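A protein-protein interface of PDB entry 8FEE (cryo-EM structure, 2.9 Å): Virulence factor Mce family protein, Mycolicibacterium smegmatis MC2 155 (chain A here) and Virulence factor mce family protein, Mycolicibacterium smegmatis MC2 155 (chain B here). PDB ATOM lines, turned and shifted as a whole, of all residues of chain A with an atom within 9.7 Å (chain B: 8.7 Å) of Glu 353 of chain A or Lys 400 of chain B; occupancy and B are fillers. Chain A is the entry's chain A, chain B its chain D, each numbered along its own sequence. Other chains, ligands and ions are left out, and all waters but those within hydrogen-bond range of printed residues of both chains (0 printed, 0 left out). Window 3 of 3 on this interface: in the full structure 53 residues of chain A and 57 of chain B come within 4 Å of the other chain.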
ATOM      1  N   LYS A 349     -11.129 -23.731  23.438  1.00  0.00           N
ATOM      2  CA  LYS A 349      -9.849 -24.161  22.891  1.00  0.00           C
ATOM      3  C   LYS A 349      -8.817 -23.067  23.122  1.00  0.00           C
ATOM      4  O   LYS A 349      -9.151 -21.928  23.450  1.00  0.00           O
ATOM      5  CB  LYS A 349      -9.941 -24.484  21.393  1.00  0.00           C
ATOM      6  CG  LYS A 349     -10.415 -25.889  21.057  1.00  0.00           C
ATOM      7  CD  LYS A 349     -10.624 -26.060  19.565  1.00  0.00           C
ATOM      8  CE  LYS A 349     -11.670 -25.092  19.051  1.00  0.00           C
ATOM      9  NZ  LYS A 349     -12.947 -25.226  19.798  1.00  0.00           N
ATOM     10  N   GLY A 350      -7.549 -23.433  22.949  1.00  0.00           N
ATOM     11  CA  GLY A 350      -6.466 -22.471  22.951  1.00  0.00           C
ATOM     12  C   GLY A 350      -6.072 -21.997  24.338  1.00  0.00           C
ATOM     13  O   GLY A 350      -6.599 -22.426  25.365  1.00  0.00           O
ATOM     14  N   GLY A 351      -5.113 -21.075  24.355  1.00  0.00           N
ATOM     15  CA  GLY A 351      -4.616 -20.503  25.584  1.00  0.00           C
ATOM     16  C   GLY A 351      -4.317 -19.024  25.440  1.00  0.00           C
ATOM     17  O   GLY A 351      -4.809 -18.359  24.524  1.00  0.00           O
ATOM     18  N   PRO A 352      -3.514 -18.476  26.350  1.00  0.00           N
ATOM     19  CA  PRO A 352      -3.176 -17.051  26.267  1.00  0.00           C
ATOM     20  C   PRO A 352      -2.327 -16.748  25.042  1.00  0.00           C
ATOM     21  O   PRO A 352      -1.476 -17.545  24.643  1.00  0.00           O
ATOM     22  CB  PRO A 352      -2.399 -16.802  27.563  1.00  0.00           C
ATOM     23  CG  PRO A 352      -1.783 -18.115  27.866  1.00  0.00           C
ATOM     24  CD  PRO A 352      -2.815 -19.138  27.464  1.00  0.00           C
ATOM     25  N   GLU A 353      -2.567 -15.572  24.454  1.00  0.00           N
ATOM     26  CA  GLU A 353      -1.887 -15.121  23.236  1.00  0.00           C
ATOM     27  C   GLU A 353      -2.128 -16.068  22.063  1.00  0.00           C
ATOM     28  O   GLU A 353      -1.282 -16.201  21.176  1.00  0.00           O
ATOM     29  CB  GLU A 353      -0.385 -14.923  23.467  1.00  0.00           C
ATOM     30  CG  GLU A 353      -0.055 -13.891  24.528  1.00  0.00           C
ATOM     31  CD  GLU A 353      -0.677 -12.538  24.242  1.00  0.00           C
ATOM     32  OE1 GLU A 353      -0.623 -12.092  23.077  1.00  0.00           O
ATOM     33  OE2 GLU A 353      -1.221 -11.922  25.181  1.00  0.00           O
ATOM     34  N   GLY A 354      -3.282 -16.732  22.048  1.00  0.00           N
ATOM     35  CA  GLY A 354      -3.664 -17.595  20.952  1.00  0.00           C
ATOM     36  C   GLY A 354      -3.144 -19.014  21.025  1.00  0.00           C
ATOM     37  O   GLY A 354      -3.630 -19.871  20.276  1.00  0.00           O
ATOM     38  N   ARG A 355      -2.183 -19.297  21.897  1.00  0.00           N
ATOM     39  CA  ARG A 355      -1.557 -20.604  21.991  1.00  0.00           C
ATOM     40  C   ARG A 355      -1.623 -21.089  23.431  1.00  0.00           C
ATOM     41  O   ARG A 355      -1.673 -20.272  24.355  1.00  0.00           O
ATOM     42  CB  ARG A 355      -0.094 -20.548  21.522  1.00  0.00           C
ATOM     43  CG  ARG A 355       0.133 -19.618  20.343  1.00  0.00           C
ATOM     44  CD  ARG A 355       1.458 -19.873  19.648  1.00  0.00           C
ATOM     45  NE  ARG A 355       2.576 -19.185  20.284  1.00  0.00           N
ATOM     46  CZ  ARG A 355       3.601 -19.797  20.859  1.00  0.00           C
ATOM     47  NH1 ARG A 355       3.669 -21.118  20.925  1.00  0.00           N
ATOM     48  NH2 ARG A 355       4.584 -19.069  21.377  1.00  0.00           N
ATOM     49  N   PRO A 356      -1.633 -22.404  23.658  1.00  0.00           N
ATOM     50  CA  PRO A 356      -1.679 -22.902  25.039  1.00  0.00           C
ATOM     51  C   PRO A 356      -0.414 -22.543  25.804  1.00  0.00           C
ATOM     52  O   PRO A 356       0.688 -22.543  25.254  1.00  0.00           O
ATOM     53  CB  PRO A 356      -1.825 -24.417  24.865  1.00  0.00           C
ATOM     54  CG  PRO A 356      -1.209 -24.694  23.546  1.00  0.00           C
ATOM     55  CD  PRO A 356      -1.552 -23.510  22.686  1.00  0.00           C
ATOM     56  N   GLY A 357      -0.588 -22.244  27.086  1.00  0.00           N
ATOM     57  CA  GLY A 357       0.529 -21.854  27.921  1.00  0.00           C
ATOM     58  C   GLY A 357       0.034 -21.247  29.219  1.00  0.00           C
ATOM     59  O   GLY A 357      -1.153 -21.314  29.546  1.00  0.00           O
ATOM     60  N   CYS A 358       0.973 -20.654  29.953  1.00  0.00           N
ATOM     61  CA  CYS A 358       0.670 -19.953  31.191  1.00  0.00           C
ATOM     62  C   CYS A 358       1.266 -18.556  31.151  1.00  0.00           C
ATOM     63  O   CYS A 358       2.265 -18.308  30.472  1.00  0.00           O
ATOM     64  CB  CYS A 358       1.226 -20.676  32.424  1.00  0.00           C
ATOM     65  SG  CYS A 358       0.865 -22.432  32.588  1.00  0.00           S
ATOM     66  N   TRP A 359       0.642 -17.643  31.892  1.00  0.00           N
ATOM     67  CA  TRP A 359       1.237 -16.341  32.140  1.00  0.00           C
ATOM     68  C   TRP A 359       2.494 -16.493  32.997  1.00  0.00           C
ATOM     69  O   TRP A 359       2.817 -17.575  33.495  1.00  0.00           O
ATOM     70  CB  TRP A 359       0.247 -15.416  32.849  1.00  0.00           C
ATOM     71  CG  TRP A 359      -1.110 -15.327  32.218  1.00  0.00           C
ATOM     72  CD1 TRP A 359      -2.269 -15.871  32.689  1.00  0.00           C
ATOM     73  CD2 TRP A 359      -1.458 -14.624  31.019  1.00  0.00           C
ATOM     74  NE1 TRP A 359      -3.312 -15.565  31.851  1.00  0.00           N
ATOM     75  CE2 TRP A 359      -2.840 -14.800  30.819  1.00  0.00           C
ATOM     76  CE3 TRP A 359      -0.732 -13.871  30.092  1.00  0.00           C
ATOM     77  CZ2 TRP A 359      -3.511 -14.250  29.730  1.00  0.00           C
ATOM     78  CZ3 TRP A 359      -1.400 -13.326  29.013  1.00  0.00           C
ATOM     79  CH2 TRP A 359      -2.774 -13.517  28.842  1.00  0.00           C
ATOM     80  N   GLN A 360       3.205 -15.385  33.184  1.00  0.00           N
ATOM     81  CA  GLN A 360       4.200 -15.337  34.237  1.00  0.00           C
ATOM     82  C   GLN A 360       3.497 -15.277  35.592  1.00  0.00           C
ATOM     83  O   GLN A 360       2.327 -14.893  35.670  1.00  0.00           O
ATOM     84  CB  GLN A 360       5.121 -14.135  34.042  1.00  0.00           C
ATOM     85  CG  GLN A 360       6.236 -14.387  33.045  1.00  0.00           C
ATOM     86  CD  GLN A 360       7.396 -13.427  33.211  1.00  0.00           C
ATOM     87  OE1 GLN A 360       7.490 -12.718  34.212  1.00  0.00           O
ATOM     88  NE2 GLN A 360       8.289 -13.403  32.230  1.00  0.00           N
ATOM     89  N   PRO A 370      -4.882 -11.273  33.238  1.00  0.00           N
ATOM     90  CA  PRO A 370      -5.544 -10.941  31.970  1.00  0.00           C
ATOM     91  C   PRO A 370      -6.666 -11.925  31.684  1.00  0.00           C
ATOM     92  O   PRO A 370      -6.439 -13.130  31.557  1.00  0.00           O
ATOM     93  CB  PRO A 370      -4.410 -11.044  30.946  1.00  0.00           C
ATOM     94  CG  PRO A 370      -3.175 -10.801  31.737  1.00  0.00           C
ATOM     95  CD  PRO A 370      -3.428 -11.428  33.076  1.00  0.00           C
ATOM     96  N   TYR A 371      -7.887 -11.402  31.607  1.00  0.00           N
ATOM     97  CA  TYR A 371      -9.063 -12.244  31.431  1.00  0.00           C
ATOM     98  C   TYR A 371      -8.981 -13.013  30.118  1.00  0.00           C
ATOM     99  O   TYR A 371      -8.509 -12.492  29.104  1.00  0.00           O
ATOM    100  CB  TYR A 371     -10.332 -11.394  31.477  1.00  0.00           C
ATOM    101  CG  TYR A 371     -11.603 -12.203  31.529  1.00  0.00           C
ATOM    102  CD1 TYR A 371     -12.138 -12.601  32.742  1.00  0.00           C
ATOM    103  CD2 TYR A 371     -12.275 -12.559  30.371  1.00  0.00           C
ATOM    104  CE1 TYR A 371     -13.299 -13.341  32.803  1.00  0.00           C
ATOM    105  CE2 TYR A 371     -13.440 -13.298  30.422  1.00  0.00           C
ATOM    106  CZ  TYR A 371     -13.948 -13.685  31.638  1.00  0.00           C
ATOM    107  OH  TYR A 371     -15.109 -14.423  31.694  1.00  0.00           O
ATOM    108  N   LEU A 372      -9.435 -14.263  30.142  1.00  0.00           N
ATOM    109  CA  LEU A 372      -9.430 -15.127  28.970  1.00  0.00           C
ATOM    110  C   LEU A 372     -10.863 -15.462  28.579  1.00  0.00           C
ATOM    111  O   LEU A 372     -11.640 -15.945  29.409  1.00  0.00           O
ATOM    112  CB  LEU A 372      -8.638 -16.408  29.234  1.00  0.00           C
ATOM    113  CG  LEU A 372      -7.936 -17.024  28.024  1.00  0.00           C
ATOM    114  CD1 LEU A 372      -6.803 -16.128  27.562  1.00  0.00           C
ATOM    115  CD2 LEU A 372      -7.419 -18.412  28.351  1.00  0.00           C
ATOM    116  N   VAL A 373     -11.203 -15.204  27.320  1.00  0.00           N
ATOM    117  CA  VAL A 373     -12.522 -15.501  26.772  1.00  0.00           C
ATOM    118  C   VAL A 373     -12.420 -16.737  25.887  1.00  0.00           C
ATOM    119  O   VAL A 373     -11.493 -16.862  25.076  1.00  0.00           O
ATOM    120  CB  VAL A 373     -13.096 -14.298  25.999  1.00  0.00           C
ATOM    121  CG1 VAL A 373     -13.325 -13.131  26.935  1.00  0.00           C
ATOM    122  CG2 VAL A 373     -12.157 -13.865  24.884  1.00  0.00           C
ATOM    123  N   ASP A 375     -14.890 -20.141  23.936  1.00  0.00           N
ATOM    124  CA  ASP A 375     -16.198 -20.461  23.365  1.00  0.00           C
ATOM    125  C   ASP A 375     -17.012 -21.203  24.414  1.00  0.00           C
ATOM    126  O   ASP A 375     -16.878 -22.417  24.581  1.00  0.00           O
ATOM    127  CB  ASP A 375     -16.041 -21.298  22.101  1.00  0.00           C
ATOM    128  CG  ASP A 375     -15.535 -20.491  20.928  1.00  0.00           C
ATOM    129  OD1 ASP A 375     -15.545 -19.246  21.015  1.00  0.00           O
ATOM    130  OD2 ASP A 375     -15.133 -21.103  19.916  1.00  0.00           O
ATOM    131  N   GLN B 394      -7.330  -5.431  29.830  1.00  0.00           N
ATOM    132  CA  GLN B 394      -7.147  -6.687  30.542  1.00  0.00           C
ATOM    133  C   GLN B 394      -7.701  -7.901  29.810  1.00  0.00           C
ATOM    134  O   GLN B 394      -7.373  -9.028  30.192  1.00  0.00           O
ATOM    135  CB  GLN B 394      -7.794  -6.604  31.932  1.00  0.00           C
ATOM    136  CG  GLN B 394      -7.089  -5.662  32.891  1.00  0.00           C
ATOM    137  CD  GLN B 394      -7.839  -5.500  34.196  1.00  0.00           C
ATOM    138  OE1 GLN B 394      -8.795  -6.224  34.466  1.00  0.00           O
ATOM    139  NE2 GLN B 394      -7.410  -4.545  35.011  1.00  0.00           N
ATOM    140  N   ILE B 395      -8.525  -7.716  28.784  1.00  0.00           N
ATOM    141  CA  ILE B 395      -9.139  -8.848  28.097  1.00  0.00           C
ATOM    142  C   ILE B 395      -8.120  -9.476  27.156  1.00  0.00           C
ATOM    143  O   ILE B 395      -7.483  -8.780  26.357  1.00  0.00           O
ATOM    144  CB  ILE B 395     -10.396  -8.408  27.334  1.00  0.00           C
ATOM    145  CG1 ILE B 395     -11.283  -7.541  28.227  1.00  0.00           C
ATOM    146  CG2 ILE B 395     -11.165  -9.620  26.842  1.00  0.00           C
ATOM    147  CD1 ILE B 395     -11.988  -8.309  29.315  1.00  0.00           C
ATOM    148  N   ALA B 396      -7.969 -10.796  27.243  1.00  0.00           N
ATOM    149  CA  ALA B 396      -7.133 -11.562  26.331  1.00  0.00           C
ATOM    150  C   ALA B 396      -7.963 -12.680  25.719  1.00  0.00           C
ATOM    151  O   ALA B 396      -8.860 -13.229  26.363  1.00  0.00           O
ATOM    152  CB  ALA B 396      -5.905 -12.144  27.035  1.00  0.00           C
ATOM    153  N   TYR B 397      -7.660 -13.010  24.469  1.00  0.00           N
ATOM    154  CA  TYR B 397      -8.490 -13.904  23.672  1.00  0.00           C
ATOM    155  C   TYR B 397      -7.805 -15.256  23.527  1.00  0.00           C
ATOM    156  O   TYR B 397      -6.618 -15.321  23.187  1.00  0.00           O
ATOM    157  CB  TYR B 397      -8.771 -13.289  22.300  1.00  0.00           C
ATOM    158  CG  TYR B 397      -9.293 -11.875  22.395  1.00  0.00           C
ATOM    159  CD1 TYR B 397     -10.627 -11.623  22.681  1.00  0.00           C
ATOM    160  CD2 TYR B 397      -8.447 -10.789  22.215  1.00  0.00           C
ATOM    161  CE1 TYR B 397     -11.104 -10.334  22.780  1.00  0.00           C
ATOM    162  CE2 TYR B 397      -8.915  -9.496  22.310  1.00  0.00           C
ATOM    163  CZ  TYR B 397     -10.244  -9.274  22.592  1.00  0.00           C
ATOM    164  OH  TYR B 397     -10.712  -7.984  22.686  1.00  0.00           O
ATOM    165  N   SER B 398      -8.558 -16.327  23.796  1.00  0.00           N
ATOM    166  CA  SER B 398      -7.987 -17.670  23.776  1.00  0.00           C
ATOM    167  C   SER B 398      -7.503 -18.048  22.382  1.00  0.00           C
ATOM    168  O   SER B 398      -6.416 -18.614  22.224  1.00  0.00           O
ATOM    169  CB  SER B 398      -9.014 -18.682  24.279  1.00  0.00           C
ATOM    170  OG  SER B 398      -8.416 -19.944  24.497  1.00  0.00           O
ATOM    171  N   GLU B 399      -8.301 -17.752  21.362  1.00  0.00           N
ATOM    172  CA  GLU B 399      -7.965 -18.043  19.976  1.00  0.00           C
ATOM    173  C   GLU B 399      -7.942 -16.739  19.195  1.00  0.00           C
ATOM    174  O   GLU B 399      -8.832 -15.898  19.358  1.00  0.00           O
ATOM    175  CB  GLU B 399      -8.979 -19.007  19.354  1.00  0.00           C
ATOM    176  CG  GLU B 399      -9.279 -20.231  20.203  1.00  0.00           C
ATOM    177  CD  GLU B 399     -10.723 -20.680  20.088  1.00  0.00           C
ATOM    178  OE1 GLU B 399     -11.181 -20.939  18.956  1.00  0.00           O
ATOM    179  OE2 GLU B 399     -11.404 -20.765  21.130  1.00  0.00           O
ATOM    180  N   LYS B 400      -6.925 -16.573  18.345  1.00  0.00           N
ATOM    181  CA  LYS B 400      -6.749 -15.310  17.635  1.00  0.00           C
ATOM    182  C   LYS B 400      -7.898 -14.999  16.686  1.00  0.00           C
ATOM    183  O   LYS B 400      -8.013 -13.854  16.235  1.00  0.00           O
ATOM    184  CB  LYS B 400      -5.429 -15.320  16.863  1.00  0.00           C
ATOM    185  CG  LYS B 400      -4.209 -15.093  17.737  1.00  0.00           C
ATOM    186  CD  LYS B 400      -2.950 -14.930  16.904  1.00  0.00           C
ATOM    187  CE  LYS B 400      -1.768 -14.528  17.769  1.00  0.00           C
ATOM    188  NZ  LYS B 400      -1.478 -15.539  18.823  1.00  0.00           N
ATOM    189  N   ARG B 401      -8.743 -15.981  16.371  1.00  0.00           N
ATOM    190  CA  ARG B 401      -9.934 -15.746  15.570  1.00  0.00           C
ATOM    191  C   ARG B 401     -11.044 -15.065  16.356  1.00  0.00           C
ATOM    192  O   ARG B 401     -12.025 -14.622  15.751  1.00  0.00           O
ATOM    193  CB  ARG B 401     -10.457 -17.067  15.007  1.00  0.00           C
ATOM    194  CG  ARG B 401     -11.173 -17.911  16.041  1.00  0.00           C
ATOM    195  CD  ARG B 401     -11.732 -19.183  15.443  1.00  0.00           C
ATOM    196  NE  ARG B 401     -12.328 -20.033  16.465  1.00  0.00           N
ATOM    197  CZ  ARG B 401     -13.536 -19.852  16.980  1.00  0.00           C
ATOM    198  NH1 ARG B 401     -14.309 -18.852  16.592  1.00  0.00           N
ATOM    199  NH2 ARG B 401     -13.979 -20.695  17.907  1.00  0.00           N
ATOM    200  N   LEU B 402     -10.918 -14.978  17.680  1.00  0.00           N
ATOM    201  CA  LEU B 402     -11.938 -14.365  18.517  1.00  0.00           C
ATOM    202  C   LEU B 402     -11.708 -12.880  18.756  1.00  0.00           C
ATOM    203  O   LEU B 402     -12.584 -12.218  19.323  1.00  0.00           O
ATOM    204  CB  LEU B 402     -12.012 -15.088  19.865  1.00  0.00           C
ATOM    205  CG  LEU B 402     -12.837 -16.373  19.907  1.00  0.00           C
ATOM    206  CD1 LEU B 402     -12.490 -17.189  21.136  1.00  0.00           C
ATOM    207  CD2 LEU B 402     -14.319 -16.045  19.884  1.00  0.00           C
ATOM    208  N   GLN B 403     -10.570 -12.344  18.346  1.00  0.00           N
ATOM    209  CA  GLN B 403     -10.251 -10.951  18.628  1.00  0.00           C
ATOM    210  C   GLN B 403     -11.074 -10.039  17.731  1.00  0.00           C
ATOM    211  O   GLN B 403     -11.027 -10.191  16.503  1.00  0.00           O
ATOM    212  CB  GLN B 403      -8.762 -10.703  18.419  1.00  0.00           C
ATOM    213  CG  GLN B 403      -8.354  -9.250  18.543  1.00  0.00           C
ATOM    214  CD  GLN B 403      -6.858  -9.066  18.437  1.00  0.00           C
ATOM    215  OE1 GLN B 403      -6.129 -10.003  18.116  1.00  0.00           O
ATOM    216  NE2 GLN B 403      -6.391  -7.853  18.709  1.00  0.00           N
ATOM    217  N   PRO B 404     -11.844  -9.104  18.283  1.00  0.00           N
ATOM    218  CA  PRO B 404     -12.691  -8.243  17.455  1.00  0.00           C
ATOM    219  C   PRO B 404     -11.859  -7.376  16.528  1.00  0.00           C
ATOM    220  O   PRO B 404     -10.773  -6.911  16.902  1.00  0.00           O
ATOM    221  CB  PRO B 404     -13.443  -7.390  18.488  1.00  0.00           C
ATOM    222  CG  PRO B 404     -13.406  -8.194  19.737  1.00  0.00           C
ATOM    223  CD  PRO B 404     -12.072  -8.877  19.717  1.00  0.00           C
ATOM    224  N   PRO B 405     -12.338  -7.136  15.313  1.00  0.00           N
ATOM    225  CA  PRO B 405     -11.651  -6.215  14.411  1.00  0.00           C
ATOM    226  C   PRO B 405     -11.917  -4.780  14.830  1.00  0.00           C
ATOM    227  O   PRO B 405     -12.760  -4.542  15.709  1.00  0.00           O
ATOM    228  CB  PRO B 405     -12.282  -6.536  13.049  1.00  0.00           C
ATOM    229  CG  PRO B 405     -13.660  -6.972  13.389  1.00  0.00           C
ATOM    230  CD  PRO B 405     -13.562  -7.690  14.711  1.00  0.00           C
ATOM    231  N   TRP B 417     -19.818 -10.124  18.101  1.00  0.00           N
ATOM    232  CA  TRP B 417     -19.218  -8.804  18.206  1.00  0.00           C
ATOM    233  C   TRP B 417     -20.267  -7.751  17.882  1.00  0.00           C
ATOM    234  O   TRP B 417     -21.007  -7.894  16.906  1.00  0.00           O
ATOM    235  CB  TRP B 417     -18.029  -8.676  17.255  1.00  0.00           C
ATOM    236  CG  TRP B 417     -16.939  -9.651  17.541  1.00  0.00           C
ATOM    237  CD1 TRP B 417     -16.577 -10.140  18.760  1.00  0.00           C
ATOM    238  CD2 TRP B 417     -16.085 -10.285  16.585  1.00  0.00           C
ATOM    239  NE1 TRP B 417     -15.538 -11.026  18.625  1.00  0.00           N
ATOM    240  CE2 TRP B 417     -15.219 -11.134  17.297  1.00  0.00           C
ATOM    241  CE3 TRP B 417     -15.965 -10.211  15.194  1.00  0.00           C
ATOM    242  CZ2 TRP B 417     -14.246 -11.904  16.668  1.00  0.00           C
ATOM    243  CZ3 TRP B 417     -14.996 -10.975  14.571  1.00  0.00           C
ATOM    244  CH2 TRP B 417     -14.150 -11.810  15.307  1.00  0.00           C
ATOM    245  N   ALA B 435     -18.172 -14.282  15.081  1.00  0.00           N
ATOM    246  CA  ALA B 435     -16.841 -14.828  14.873  1.00  0.00           C
ATOM    247  C   ALA B 435     -16.916 -16.059  13.968  1.00  0.00           C
ATOM    248  O   ALA B 435     -17.936 -16.755  13.941  1.00  0.00           O
ATOM    249  CB  ALA B 435     -16.196 -15.197  16.208  1.00  0.00           C
ATOM    250  N   PRO B 436     -15.862 -16.334  13.198  1.00  0.00           N
ATOM    251  CA  PRO B 436     -15.855 -17.542  12.364  1.00  0.00           C
ATOM    252  C   PRO B 436     -15.963 -18.808  13.202  1.00  0.00           C
ATOM    253  O   PRO B 436     -15.430 -18.892  14.309  1.00  0.00           O
ATOM    254  CB  PRO B 436     -14.508 -17.463  11.638  1.00  0.00           C
ATOM    255  CG  PRO B 436     -14.155 -16.015  11.651  1.00  0.00           C
ATOM    256  CD  PRO B 436     -14.689 -15.481  12.945  1.00  0.00           C
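Of the printed residues of chain B, Glu 353 of chain A touches Lys 400.
Of the printed residues of chain B, Trp 359 of chain A touches Ala 396.
Of the printed residues of chain B, Leu 372 of chain A touches Ala 396 (3.3 Å).
Of the printed residues of chain A, Ile 395 of chain B touches Tyr 371.
Lys 400 of chain B touches just these residues of chain A: Glu 353 and Gly 354.
Pro 404 of chain B touches none of the printed residues of chain A.
The nearest residue of chain B that does not touch Glu 353 of chain A is Tyr 397 of chain B (4.3 Å).
Gly 351 of chain A touches Tyr 397 of chain B.
Gly 354 of chain A touches Tyr 397 of chain B (N to O, 3.8 Å).
O of Ser 398 of chain B touches CA of Gly 354 of chain A, 3.2 Å away.
CH2 of Trp 359 of chain A touches CB of Ala 396 of chain B (3.9 Å).
Pro 370 of chain A touches Gln 394 of chain B.
Ile 395 of chain B touches Tyr 371 of chain A.
O of Ala 396 of chain B touches CA of Leu 372 of chain A, at 3.3 Å.
Val 373 of chain A touches Tyr 397 of chain B.
OD2 of Asp 375 of chain A touches OE2 of Glu 399 of chain B, at 3.9 Å.
Leu 402 of chain B touches Asp 375 of chain A (CD2 to OD1, 3.6 Å).
The backbone carbonyl oxygen (O) of Gly 350 of chain A sits close to the side-chain hydroxyl (OG) of Ser 398 of chain B, 3.2 Å away.
The backbone NH (N) of Gly 351 of chain A is in hydrogen-bond range of the side-chain hydroxyl (OG) of Ser 398 of chain B.
The backbone carbonyl oxygen (O) of Glu 353 of chain A is in hydrogen-bond range of the side-chain amino group (NZ) of Lys 400 of chain B, at 2.5 Å.
The backbone NH of Tyr 371 of chain A sits at hydrogen-bond distance from the backbone carbonyl oxygen of Gln 394 of chain B (2.8 Å).
The backbone carbonyl oxygen (O) of Tyr 371 of chain A lies within hydrogen-bond range of the backbone NH (N) of Ala 396 of chain B, at 2.6 Å.
The backbone NH of Val 373 of chain A lies within hydrogen-bond range of the backbone carbonyl oxygen of Ala 396 of chain B, at 3.2 Å.
The backbone carbonyl oxygen of Val 373 of chain A lies close to the backbone NH of Ser 398 of chain B (3.2 Å).
The guanidinium group (NH2) of Arg 401 of chain B lies within salt-bridge range of the side-chain carboxylate (OD1) of Asp 375 of chain A.
OG of Ser 398 of chain B sits close to O of Lys 349 of chain A (2.4 Å).
The side-chain carboxylate (OE2) of Glu 399 of chain B lies close to the backbone carbonyl oxygen (O) of Lys 349 of chain A (3.4 Å).
The guanidinium group (NE) of Arg 401 of chain B is in salt-bridge range of the side-chain carboxylate (OE1) of Glu 399 of chain B (2.9 Å).
The guanidinium group of Arg 401 of chain B sits at hydrogen-bond distance from the backbone carbonyl oxygen of Pro 436 of chain B, at 2.5 Å.
The backbone carbonyl oxygen (O) of Leu 402 of chain B sits close to the indole nitrogen (NE1) of Trp 417 of chain B, at 3.3 Å.
Printed residues of chain A that touch a printed residue of chain B: Lys 349, Gly 350, Gly 351, Glu 353, Gly 354, Trp 359, Pro 370, Tyr 371, Leu 372, Val 373 and Asp 375.
Of the 15 printed residues of chain B, 9 touch a printed residue of chain A.
Hydrophobic or aromatic side chains of chain B that line the printed part of chain A: Ala 396, Tyr 397 and Leu 402.
Along chain B the printed residues that touch a printed residue of chain A span positions 394 to 402.
Among the printed residues, Asp or Glu carboxylates within 4 Å of a Lys or Arg side-chain nitrogen of the other chain: Asp 375 of chain A with Arg 401 of chain B (2.4 Å).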
